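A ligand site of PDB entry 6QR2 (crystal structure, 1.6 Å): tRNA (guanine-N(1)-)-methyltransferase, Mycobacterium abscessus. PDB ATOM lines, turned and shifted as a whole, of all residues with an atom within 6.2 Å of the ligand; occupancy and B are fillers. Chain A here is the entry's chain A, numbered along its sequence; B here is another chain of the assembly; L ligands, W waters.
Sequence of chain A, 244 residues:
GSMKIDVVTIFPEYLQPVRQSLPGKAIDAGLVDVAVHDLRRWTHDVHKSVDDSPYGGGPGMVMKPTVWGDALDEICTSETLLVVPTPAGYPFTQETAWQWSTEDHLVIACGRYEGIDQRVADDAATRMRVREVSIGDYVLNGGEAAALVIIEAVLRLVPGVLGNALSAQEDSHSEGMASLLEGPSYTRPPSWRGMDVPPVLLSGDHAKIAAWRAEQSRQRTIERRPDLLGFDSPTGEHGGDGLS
O of Val 133 lies close to N3 of the ligand.
Residues that only touch the ligand: Pro 85 (3.3 Å), Pro 87 (3.5 Å), Gly 111 (3.4 Å), Arg 112 (3.6 Å), Tyr 113 (3.2 Å), Glu 114 (3.5 Å), Val 139 (3.6 Å), Asn 141 (3.5 Å), Gly 142 (3.6 Å), Gly 143 (3.5 Å), Ala 146 (3.5 Å) and Glu 182 of chain B (3.6 Å).
OG of Ser 134 is in hydrogen-bond range of N6 of the ligand, 3.0 Å away.
An oxygen (O1) of the ligand is in hydrogen-bond range of the guanidinium group (NH2) of Arg 156 of chain B.
The backbone NH of Ile 135 is in hydrogen-bond range of a nitrogen (N3) of the ligand, 3.5 Å away.
The backbone NH (N) of Thr 86 lies within hydrogen-bond range of a nitrogen (N3) of the ligand, 3.5 Å away.
The backbone carbonyl oxygen of Gly 136 sits at hydrogen-bond distance from a nitrogen (N6) of the ligand (3.0 Å).
The backbone carbonyl oxygen (O) of Tyr 138 sits at hydrogen-bond distance from a nitrogen (N4) of the ligand (2.6 Å).
N of Leu 140 sits at hydrogen-bond distance from N5 of the ligand (3.0 Å).
Water W1 lies within hydrogen-bond range of an oxygen (O1) of the ligand (2.7 Å), the backbone carbonyl oxygen of Tyr 113 (3.1 Å) and the side-chain carboxylate of Glu 114 (3.2 Å).
The side-chain amide oxygen (OD1) of Asn 141 sits at hydrogen-bond distance from the guanidinium group (NE) of Arg 156 of chain B.
The side-chain hydroxyl (OH) of Tyr 138 lies within hydrogen-bond range of the backbone carbonyl oxygen (O) of Ile 135 (3.2 Å).
The backbone carbonyl oxygen of Gly 143 lies within hydrogen-bond range of the side-chain sulfur of Cys 110.
The guanidinium group (NE) of Arg 112 is in salt-bridge range of the side-chain carboxylate (OE1) of Glu 144 (2.8 Å).
O of Gly 111 lies within hydrogen-bond range of N of Gly 143, 2.9 Å away.
The backbone carbonyl oxygen of Val 133 is in hydrogen-bond range of the backbone NH of Thr 86, at 2.9 Å.
The backbone carbonyl oxygen (O) of Gly 136 is in hydrogen-bond range of the side-chain hydroxyl (OG) of Ser 134.
O of Val 84 sits at hydrogen-bond distance from N of Val 133, at 3.1 Å.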
ATOM      1  N   VAL A  84      29.256 -23.823   4.440  1.00  0.00           N
ATOM      2  CA  VAL A  84      28.104 -24.641   4.075  1.00  0.00           C
ATOM      3  C   VAL A  84      26.819 -23.955   4.513  1.00  0.00           C
ATOM      4  O   VAL A  84      26.446 -24.004   5.695  1.00  0.00           O
ATOM      5  CB  VAL A  84      28.151 -26.041   4.711  1.00  0.00           C
ATOM      6  CG1 VAL A  84      26.995 -26.881   4.179  1.00  0.00           C
ATOM      7  CG2 VAL A  84      29.492 -26.728   4.412  1.00  0.00           C
ATOM      8  N   PRO A  85      26.156 -23.261   3.584  1.00  0.00           N
ATOM      9  CA  PRO A  85      24.855 -22.692   3.930  1.00  0.00           C
ATOM     10  C   PRO A  85      23.856 -23.765   4.330  1.00  0.00           C
ATOM     11  O   PRO A  85      23.795 -24.821   3.714  1.00  0.00           O
ATOM     12  CB  PRO A  85      24.422 -21.982   2.644  1.00  0.00           C
ATOM     13  CG  PRO A  85      25.734 -21.681   1.916  1.00  0.00           C
ATOM     14  CD  PRO A  85      26.587 -22.896   2.221  1.00  0.00           C
ATOM     15  N   THR A  86      23.084 -23.468   5.374  1.00  0.00           N
ATOM     16  CA  THR A  86      22.050 -24.379   5.844  1.00  0.00           C
ATOM     17  C   THR A  86      21.114 -23.618   6.772  1.00  0.00           C
ATOM     18  O   THR A  86      21.565 -22.747   7.521  1.00  0.00           O
ATOM     19  CB  THR A  86      22.629 -25.603   6.589  1.00  0.00           C
ATOM     20  OG1 THR A  86      21.591 -26.239   7.372  1.00  0.00           O
ATOM     21  CG2 THR A  86      23.793 -25.213   7.489  1.00  0.00           C
ATOM     22  N   PRO A  87      19.826 -23.935   6.719  1.00  0.00           N
ATOM     23  CA  PRO A  87      18.910 -23.252   7.638  1.00  0.00           C
ATOM     24  C   PRO A  87      19.206 -23.597   9.109  1.00  0.00           C
ATOM     25  O   PRO A  87      18.732 -22.872   9.989  1.00  0.00           O
ATOM     26  CB  PRO A  87      17.523 -23.748   7.202  1.00  0.00           C
ATOM     27  CG  PRO A  87      17.765 -24.997   6.455  1.00  0.00           C
ATOM     28  CD  PRO A  87      19.133 -24.919   5.853  1.00  0.00           C
ATOM     29  N   CYS A 110      26.969 -25.401  -1.984  1.00  0.00           N
ATOM     30  CA  CYS A 110      25.528 -25.114  -2.052  1.00  0.00           C
ATOM     31  C   CYS A 110      24.677 -26.350  -2.176  1.00  0.00           C
ATOM     32  O   CYS A 110      24.724 -27.043  -3.201  1.00  0.00           O
ATOM     33  CB  CYS A 110      25.220 -24.207  -3.229  1.00  0.00           C
ATOM     34  SG  CYS A 110      26.049 -22.608  -3.174  1.00  0.00           S
ATOM     35  N   GLY A 111      23.869 -26.618  -1.154  1.00  0.00           N
ATOM     36  CA  GLY A 111      22.944 -27.735  -1.207  1.00  0.00           C
ATOM     37  C   GLY A 111      21.631 -27.390  -1.871  1.00  0.00           C
ATOM     38  O   GLY A 111      21.317 -26.229  -2.134  1.00  0.00           O
ATOM     39  N   ARG A 112      20.889 -28.444  -2.187  1.00  0.00           N
ATOM     40  CA  ARG A 112      19.496 -28.351  -2.617  1.00  0.00           C
ATOM     41  C   ARG A 112      18.758 -29.485  -1.905  1.00  0.00           C
ATOM     42  O   ARG A 112      19.319 -30.155  -1.046  1.00  0.00           O
ATOM     43  CB  ARG A 112      19.383 -28.465  -4.142  1.00  0.00           C
ATOM     44  CG  ARG A 112      19.732 -27.179  -4.904  1.00  0.00           C
ATOM     45  CD  ARG A 112      18.482 -26.316  -5.077  1.00  0.00           C
ATOM     46  NE  ARG A 112      18.795 -24.891  -5.217  1.00  0.00           N
ATOM     47  CZ  ARG A 112      17.903 -23.975  -5.572  1.00  0.00           C
ATOM     48  NH1 ARG A 112      16.645 -24.332  -5.842  1.00  0.00           N
ATOM     49  NH2 ARG A 112      18.269 -22.694  -5.663  1.00  0.00           N
ATOM     50  N   TYR A 113      17.492 -29.695  -2.268  1.00  0.00           N
ATOM     51  CA  TYR A 113      16.647 -30.705  -1.623  1.00  0.00           C
ATOM     52  C   TYR A 113      16.605 -30.447  -0.114  1.00  0.00           C
ATOM     53  O   TYR A 113      16.372 -29.313   0.312  1.00  0.00           O
ATOM     54  CB  TYR A 113      17.158 -32.112  -1.945  1.00  0.00           C
ATOM     55  CG  TYR A 113      17.282 -32.383  -3.430  1.00  0.00           C
ATOM     56  CD1 TYR A 113      16.200 -32.854  -4.159  1.00  0.00           C
ATOM     57  CD2 TYR A 113      18.482 -32.164  -4.092  1.00  0.00           C
ATOM     58  CE1 TYR A 113      16.309 -33.106  -5.508  1.00  0.00           C
ATOM     59  CE2 TYR A 113      18.596 -32.414  -5.454  1.00  0.00           C
ATOM     60  CZ  TYR A 113      17.511 -32.884  -6.154  1.00  0.00           C
ATOM     61  OH  TYR A 113      17.628 -33.132  -7.499  1.00  0.00           O
ATOM     62  N   GLU A 114      16.820 -31.490   0.696  1.00  0.00           N
ATOM     63  CA  GLU A 114      16.771 -31.311   2.153  1.00  0.00           C
ATOM     64  C   GLU A 114      18.136 -30.995   2.750  1.00  0.00           C
ATOM     65  O   GLU A 114      18.262 -30.764   3.948  1.00  0.00           O
ATOM     66  CB  GLU A 114      16.191 -32.551   2.832  1.00  0.00           C
ATOM     67  CG  GLU A 114      14.782 -32.885   2.393  1.00  0.00           C
ATOM     68  CD  GLU A 114      13.803 -31.752   2.657  1.00  0.00           C
ATOM     69  OE1 GLU A 114      13.376 -31.095   1.691  1.00  0.00           O
ATOM     70  OE2 GLU A 114      13.466 -31.538   3.835  1.00  0.00           O
ATOM     71  N   GLY A 115      19.157 -30.964   1.901  1.00  0.00           N
ATOM     72  CA  GLY A 115      20.489 -30.636   2.354  1.00  0.00           C
ATOM     73  C   GLY A 115      21.464 -31.738   1.991  1.00  0.00           C
ATOM     74  O   GLY A 115      21.131 -32.647   1.241  1.00  0.00           O
ATOM     75  N   ILE A 116      22.661 -31.650   2.548  1.00  0.00           N
ATOM     76  CA  ILE A 116      23.756 -32.558   2.208  1.00  0.00           C
ATOM     77  C   ILE A 116      23.955 -33.561   3.333  1.00  0.00           C
ATOM     78  O   ILE A 116      23.895 -33.180   4.496  1.00  0.00           O
ATOM     79  CB  ILE A 116      25.065 -31.769   1.986  1.00  0.00           C
ATOM     80  CG1 ILE A 116      24.875 -30.677   0.923  1.00  0.00           C
ATOM     81  CG2 ILE A 116      26.215 -32.716   1.602  1.00  0.00           C
ATOM     82  CD1 ILE A 116      26.053 -29.725   0.791  1.00  0.00           C
ATOM     83  N   VAL A 133      26.510 -22.211   8.214  1.00  0.00           N
ATOM     84  CA  VAL A 133      25.927 -20.902   8.538  1.00  0.00           C
ATOM     85  C   VAL A 133      24.588 -20.696   7.876  1.00  0.00           C
ATOM     86  O   VAL A 133      24.296 -21.290   6.830  1.00  0.00           O
ATOM     87  CB  VAL A 133      26.851 -19.734   8.112  1.00  0.00           C
ATOM     88  CG1 VAL A 133      28.165 -19.728   8.923  1.00  0.00           C
ATOM     89  CG2 VAL A 133      27.120 -19.754   6.590  1.00  0.00           C
ATOM     90  N   SER A 134      23.774 -19.842   8.505  1.00  0.00           N
ATOM     91  CA  SER A 134      22.496 -19.432   7.951  1.00  0.00           C
ATOM     92  C   SER A 134      22.466 -17.927   7.769  1.00  0.00           C
ATOM     93  O   SER A 134      22.878 -17.190   8.669  1.00  0.00           O
ATOM     94  CB  SER A 134      21.363 -19.844   8.886  1.00  0.00           C
ATOM     95  OG  SER A 134      20.150 -19.214   8.512  1.00  0.00           O
ATOM     96  N   ILE A 135      21.927 -17.464   6.637  1.00  0.00           N
ATOM     97  CA  ILE A 135      21.858 -16.012   6.416  1.00  0.00           C
ATOM     98  C   ILE A 135      20.609 -15.328   7.009  1.00  0.00           C
ATOM     99  O   ILE A 135      20.492 -14.104   6.930  1.00  0.00           O
ATOM    100  CB  ILE A 135      21.961 -15.646   4.915  1.00  0.00           C
ATOM    101  CG1 ILE A 135      20.813 -16.274   4.113  1.00  0.00           C
ATOM    102  CG2 ILE A 135      23.329 -16.071   4.353  1.00  0.00           C
ATOM    103  CD1 ILE A 135      20.528 -15.532   2.793  1.00  0.00           C
ATOM    104  N   GLY A 136      19.686 -16.080   7.608  1.00  0.00           N
ATOM    105  CA  GLY A 136      18.502 -15.467   8.196  1.00  0.00           C
ATOM    106  C   GLY A 136      17.422 -16.474   8.539  1.00  0.00           C
ATOM    107  O   GLY A 136      17.501 -17.652   8.221  1.00  0.00           O
ATOM    108  N   ASP A 137      16.383 -15.980   9.211  1.00  0.00           N
ATOM    109  CA  ASP A 137      15.370 -16.859   9.755  1.00  0.00           C
ATOM    110  C   ASP A 137      14.177 -17.035   8.833  1.00  0.00           C
ATOM    111  O   ASP A 137      13.050 -16.637   9.137  1.00  0.00           O
ATOM    112  CB  ASP A 137      14.927 -16.344  11.122  1.00  0.00           C
ATOM    113  CG  ASP A 137      16.025 -16.467  12.158  1.00  0.00           C
ATOM    114  OD1 ASP A 137      16.920 -17.322  11.942  1.00  0.00           O
ATOM    115  OD2 ASP A 137      16.007 -15.745  13.168  1.00  0.00           O
ATOM    116  N   TYR A 138      14.466 -17.665   7.702  1.00  0.00           N
ATOM    117  CA  TYR A 138      13.497 -17.968   6.663  1.00  0.00           C
ATOM    118  C   TYR A 138      14.091 -19.174   5.956  1.00  0.00           C
ATOM    119  O   TYR A 138      15.284 -19.452   6.090  1.00  0.00           O
ATOM    120  CB  TYR A 138      13.283 -16.802   5.693  1.00  0.00           C
ATOM    121  CG  TYR A 138      14.557 -16.033   5.438  1.00  0.00           C
ATOM    122  CD1 TYR A 138      15.530 -16.535   4.559  1.00  0.00           C
ATOM    123  CD2 TYR A 138      14.807 -14.833   6.092  1.00  0.00           C
ATOM    124  CE1 TYR A 138      16.718 -15.868   4.363  1.00  0.00           C
ATOM    125  CE2 TYR A 138      15.989 -14.146   5.887  1.00  0.00           C
ATOM    126  CZ  TYR A 138      16.940 -14.665   5.020  1.00  0.00           C
ATOM    127  OH  TYR A 138      18.132 -14.013   4.808  1.00  0.00           O
ATOM    128  N   VAL A 139      13.258 -19.879   5.199  1.00  0.00           N
ATOM    129  CA  VAL A 139      13.696 -21.067   4.490  1.00  0.00           C
ATOM    130  C   VAL A 139      13.777 -20.807   2.996  1.00  0.00           C
ATOM    131  O   VAL A 139      12.830 -20.293   2.386  1.00  0.00           O
ATOM    132  CB  VAL A 139      12.741 -22.232   4.749  1.00  0.00           C
ATOM    133  CG1 VAL A 139      13.264 -23.494   4.073  1.00  0.00           C
ATOM    134  CG2 VAL A 139      12.571 -22.441   6.243  1.00  0.00           C
ATOM    135  N   LEU A 140      14.935 -21.140   2.412  1.00  0.00           N
ATOM    136  CA  LEU A 140      15.152 -21.045   0.970  1.00  0.00           C
ATOM    137  C   LEU A 140      15.040 -22.421   0.327  1.00  0.00           C
ATOM    138  O   LEU A 140      14.894 -23.412   1.037  1.00  0.00           O
ATOM    139  CB  LEU A 140      16.527 -20.432   0.705  1.00  0.00           C
ATOM    140  CG  LEU A 140      16.759 -19.061   1.336  1.00  0.00           C
ATOM    141  CD1 LEU A 140      18.219 -18.689   1.206  1.00  0.00           C
ATOM    142  CD2 LEU A 140      15.890 -18.007   0.662  1.00  0.00           C
ATOM    143  N   ASN A 141      15.130 -22.491  -1.006  1.00  0.00           N
ATOM    144  CA  ASN A 141      15.133 -23.797  -1.683  1.00  0.00           C
ATOM    145  C   ASN A 141      16.506 -24.458  -1.725  1.00  0.00           C
ATOM    146  O   ASN A 141      16.611 -25.652  -2.004  1.00  0.00           O
ATOM    147  CB  ASN A 141      14.632 -23.669  -3.107  1.00  0.00           C
ATOM    148  CG  ASN A 141      13.156 -23.384  -3.175  1.00  0.00           C
ATOM    149  OD1 ASN A 141      12.368 -23.970  -2.427  1.00  0.00           O
ATOM    150  ND2 ASN A 141      12.767 -22.480  -4.061  1.00  0.00           N
ATOM    151  N   GLY A 142      17.551 -23.678  -1.480  1.00  0.00           N
ATOM    152  CA  GLY A 142      18.905 -24.187  -1.595  1.00  0.00           C
ATOM    153  C   GLY A 142      19.896 -23.130  -1.188  1.00  0.00           C
ATOM    154  O   GLY A 142      19.517 -22.009  -0.826  1.00  0.00           O
ATOM    155  N   GLY A 143      21.173 -23.470  -1.282  1.00  0.00           N
ATOM    156  CA  GLY A 143      22.219 -22.599  -0.784  1.00  0.00           C
ATOM    157  C   GLY A 143      22.677 -21.476  -1.693  1.00  0.00           C
ATOM    158  O   GLY A 143      23.455 -20.624  -1.257  1.00  0.00           O
ATOM    159  N   GLU A 144      22.221 -21.455  -2.943  1.00  0.00           N
ATOM    160  CA  GLU A 144      22.724 -20.498  -3.940  1.00  0.00           C
ATOM    161  C   GLU A 144      22.452 -19.040  -3.580  1.00  0.00           C
ATOM    162  O   GLU A 144      23.354 -18.214  -3.668  1.00  0.00           O
ATOM    163  CB  GLU A 144      22.151 -20.813  -5.315  1.00  0.00           C
ATOM    164  CG  GLU A 144      22.715 -22.082  -5.943  1.00  0.00           C
ATOM    165  CD  GLU A 144      22.072 -23.374  -5.430  1.00  0.00           C
ATOM    166  OE1 GLU A 144      21.063 -23.312  -4.703  1.00  0.00           O
ATOM    167  OE2 GLU A 144      22.593 -24.454  -5.773  1.00  0.00           O
ATOM    168  N   ALA A 146      21.973 -17.890  -0.673  1.00  0.00           N
ATOM    169  CA  ALA A 146      22.788 -17.613   0.506  1.00  0.00           C
ATOM    170  C   ALA A 146      24.241 -17.361   0.094  1.00  0.00           C
ATOM    171  O   ALA A 146      24.895 -16.475   0.644  1.00  0.00           O
ATOM    172  CB  ALA A 146      22.711 -18.787   1.499  1.00  0.00           C
ATOM    173  N   ILE A 150      26.449 -14.090   1.011  1.00  0.00           N
ATOM    174  CA  ILE A 150      27.743 -14.239   1.678  1.00  0.00           C
ATOM    175  C   ILE A 150      28.877 -13.645   0.844  1.00  0.00           C
ATOM    176  O   ILE A 150      29.702 -12.883   1.357  1.00  0.00           O
ATOM    177  CB  ILE A 150      28.022 -15.723   1.983  1.00  0.00           C
ATOM    178  CG1 ILE A 150      27.035 -16.219   3.038  1.00  0.00           C
ATOM    179  CG2 ILE A 150      29.487 -15.945   2.433  1.00  0.00           C
ATOM    180  CD1 ILE A 150      27.014 -17.714   3.161  1.00  0.00           C
ATOM    181  N   ARG B 156       8.172 -20.107  -2.637  1.00  0.00           N
ATOM    182  CA  ARG B 156       8.041 -21.514  -2.286  1.00  0.00           C
ATOM    183  C   ARG B 156       6.791 -21.773  -1.402  1.00  0.00           C
ATOM    184  O   ARG B 156       6.388 -22.922  -1.202  1.00  0.00           O
ATOM    185  CB  ARG B 156       9.311 -22.038  -1.618  1.00  0.00           C
ATOM    186  CG  ARG B 156       9.715 -21.356  -0.342  1.00  0.00           C
ATOM    187  CD  ARG B 156      11.122 -21.798   0.085  1.00  0.00           C
ATOM    188  NE  ARG B 156      11.204 -23.230   0.383  1.00  0.00           N
ATOM    189  CZ  ARG B 156      10.732 -23.808   1.483  1.00  0.00           C
ATOM    190  NH1 ARG B 156      10.114 -23.080   2.403  1.00  0.00           N
ATOM    191  NH2 ARG B 156      10.865 -25.105   1.659  1.00  0.00           N
ATOM    192  N   GLU B 182      16.658 -27.741  12.093  1.00  0.00           N
ATOM    193  CA  GLU B 182      16.691 -29.085  11.547  1.00  0.00           C
ATOM    194  C   GLU B 182      17.919 -29.858  12.017  1.00  0.00           C
ATOM    195  O   GLU B 182      19.013 -29.294  12.122  1.00  0.00           O
ATOM    196  CB  GLU B 182      16.662 -29.048  10.016  1.00  0.00           C
ATOM    197  CG  GLU B 182      15.407 -28.448   9.411  1.00  0.00           C
ATOM    198  CD  GLU B 182      14.336 -29.487   9.144  1.00  0.00           C
ATOM    199  OE1 GLU B 182      14.091 -30.334  10.025  1.00  0.00           O
ATOM    200  OE2 GLU B 182      13.752 -29.455   8.042  1.00  0.00           O
HETATM  201  C1  LIG L   1      18.674 -27.085   0.834  1.00  0.00           C
HETATM  202  C2  LIG L   1      18.587 -25.105   1.884  1.00  0.00           C
HETATM  203  C3  LIG L   1      19.184 -23.000   2.938  1.00  0.00           C
HETATM  204  C4  LIG L   1      20.966 -24.420   2.084  1.00  0.00           C
HETATM  205  C5  LIG L   1      20.928 -20.537   4.486  1.00  0.00           C
HETATM  206  C6  LIG L   1      18.511 -20.030   5.033  1.00  0.00           C
HETATM  207  O1  LIG L   1      13.683 -26.853   1.834  1.00  0.00           O
HETATM  208  C7  LIG L   1      14.599 -27.249   2.857  1.00  0.00           C
HETATM  209  N1  LIG L   1      14.142 -27.838   3.915  1.00  0.00           N
HETATM  210  C8  LIG L   1      14.968 -28.218   4.901  1.00  0.00           C
HETATM  211  C9  LIG L   1      16.353 -27.990   4.829  1.00  0.00           C
HETATM  212  C10 LIG L   1      16.882 -27.354   3.700  1.00  0.00           C
HETATM  213  C11 LIG L   1      15.967 -26.965   2.684  1.00  0.00           C
HETATM  214  C12 LIG L   1      16.418 -26.274   1.428  1.00  0.00           C
HETATM  215  N2  LIG L   1      17.862 -26.164   1.388  1.00  0.00           N
HETATM  216  C13 LIG L   1      20.010 -26.619   0.982  1.00  0.00           C
HETATM  217  C14 LIG L   1      19.959 -25.353   1.649  1.00  0.00           C
HETATM  218  C15 LIG L   1      18.185 -23.918   2.546  1.00  0.00           C
HETATM  219  C16 LIG L   1      20.581 -23.243   2.722  1.00  0.00           C
HETATM  220  C17 LIG L   1      18.734 -21.805   3.713  1.00  0.00           C
HETATM  221  C18 LIG L   1      19.458 -20.827   4.398  1.00  0.00           C
HETATM  222  N3  LIG L   1      22.040 -20.256   4.584  1.00  0.00           N
HETATM  223  N4  LIG L   1      17.269 -20.530   4.758  1.00  0.00           N
HETATM  224  N5  LIG L   1      17.413 -21.616   3.984  1.00  0.00           N
HETATM  225  N6  LIG L   1      18.774 -18.867   5.850  1.00  0.00           N
HETATM  226  O   HOH W   1      13.438 -28.579  -0.289  1.00  0.00           O
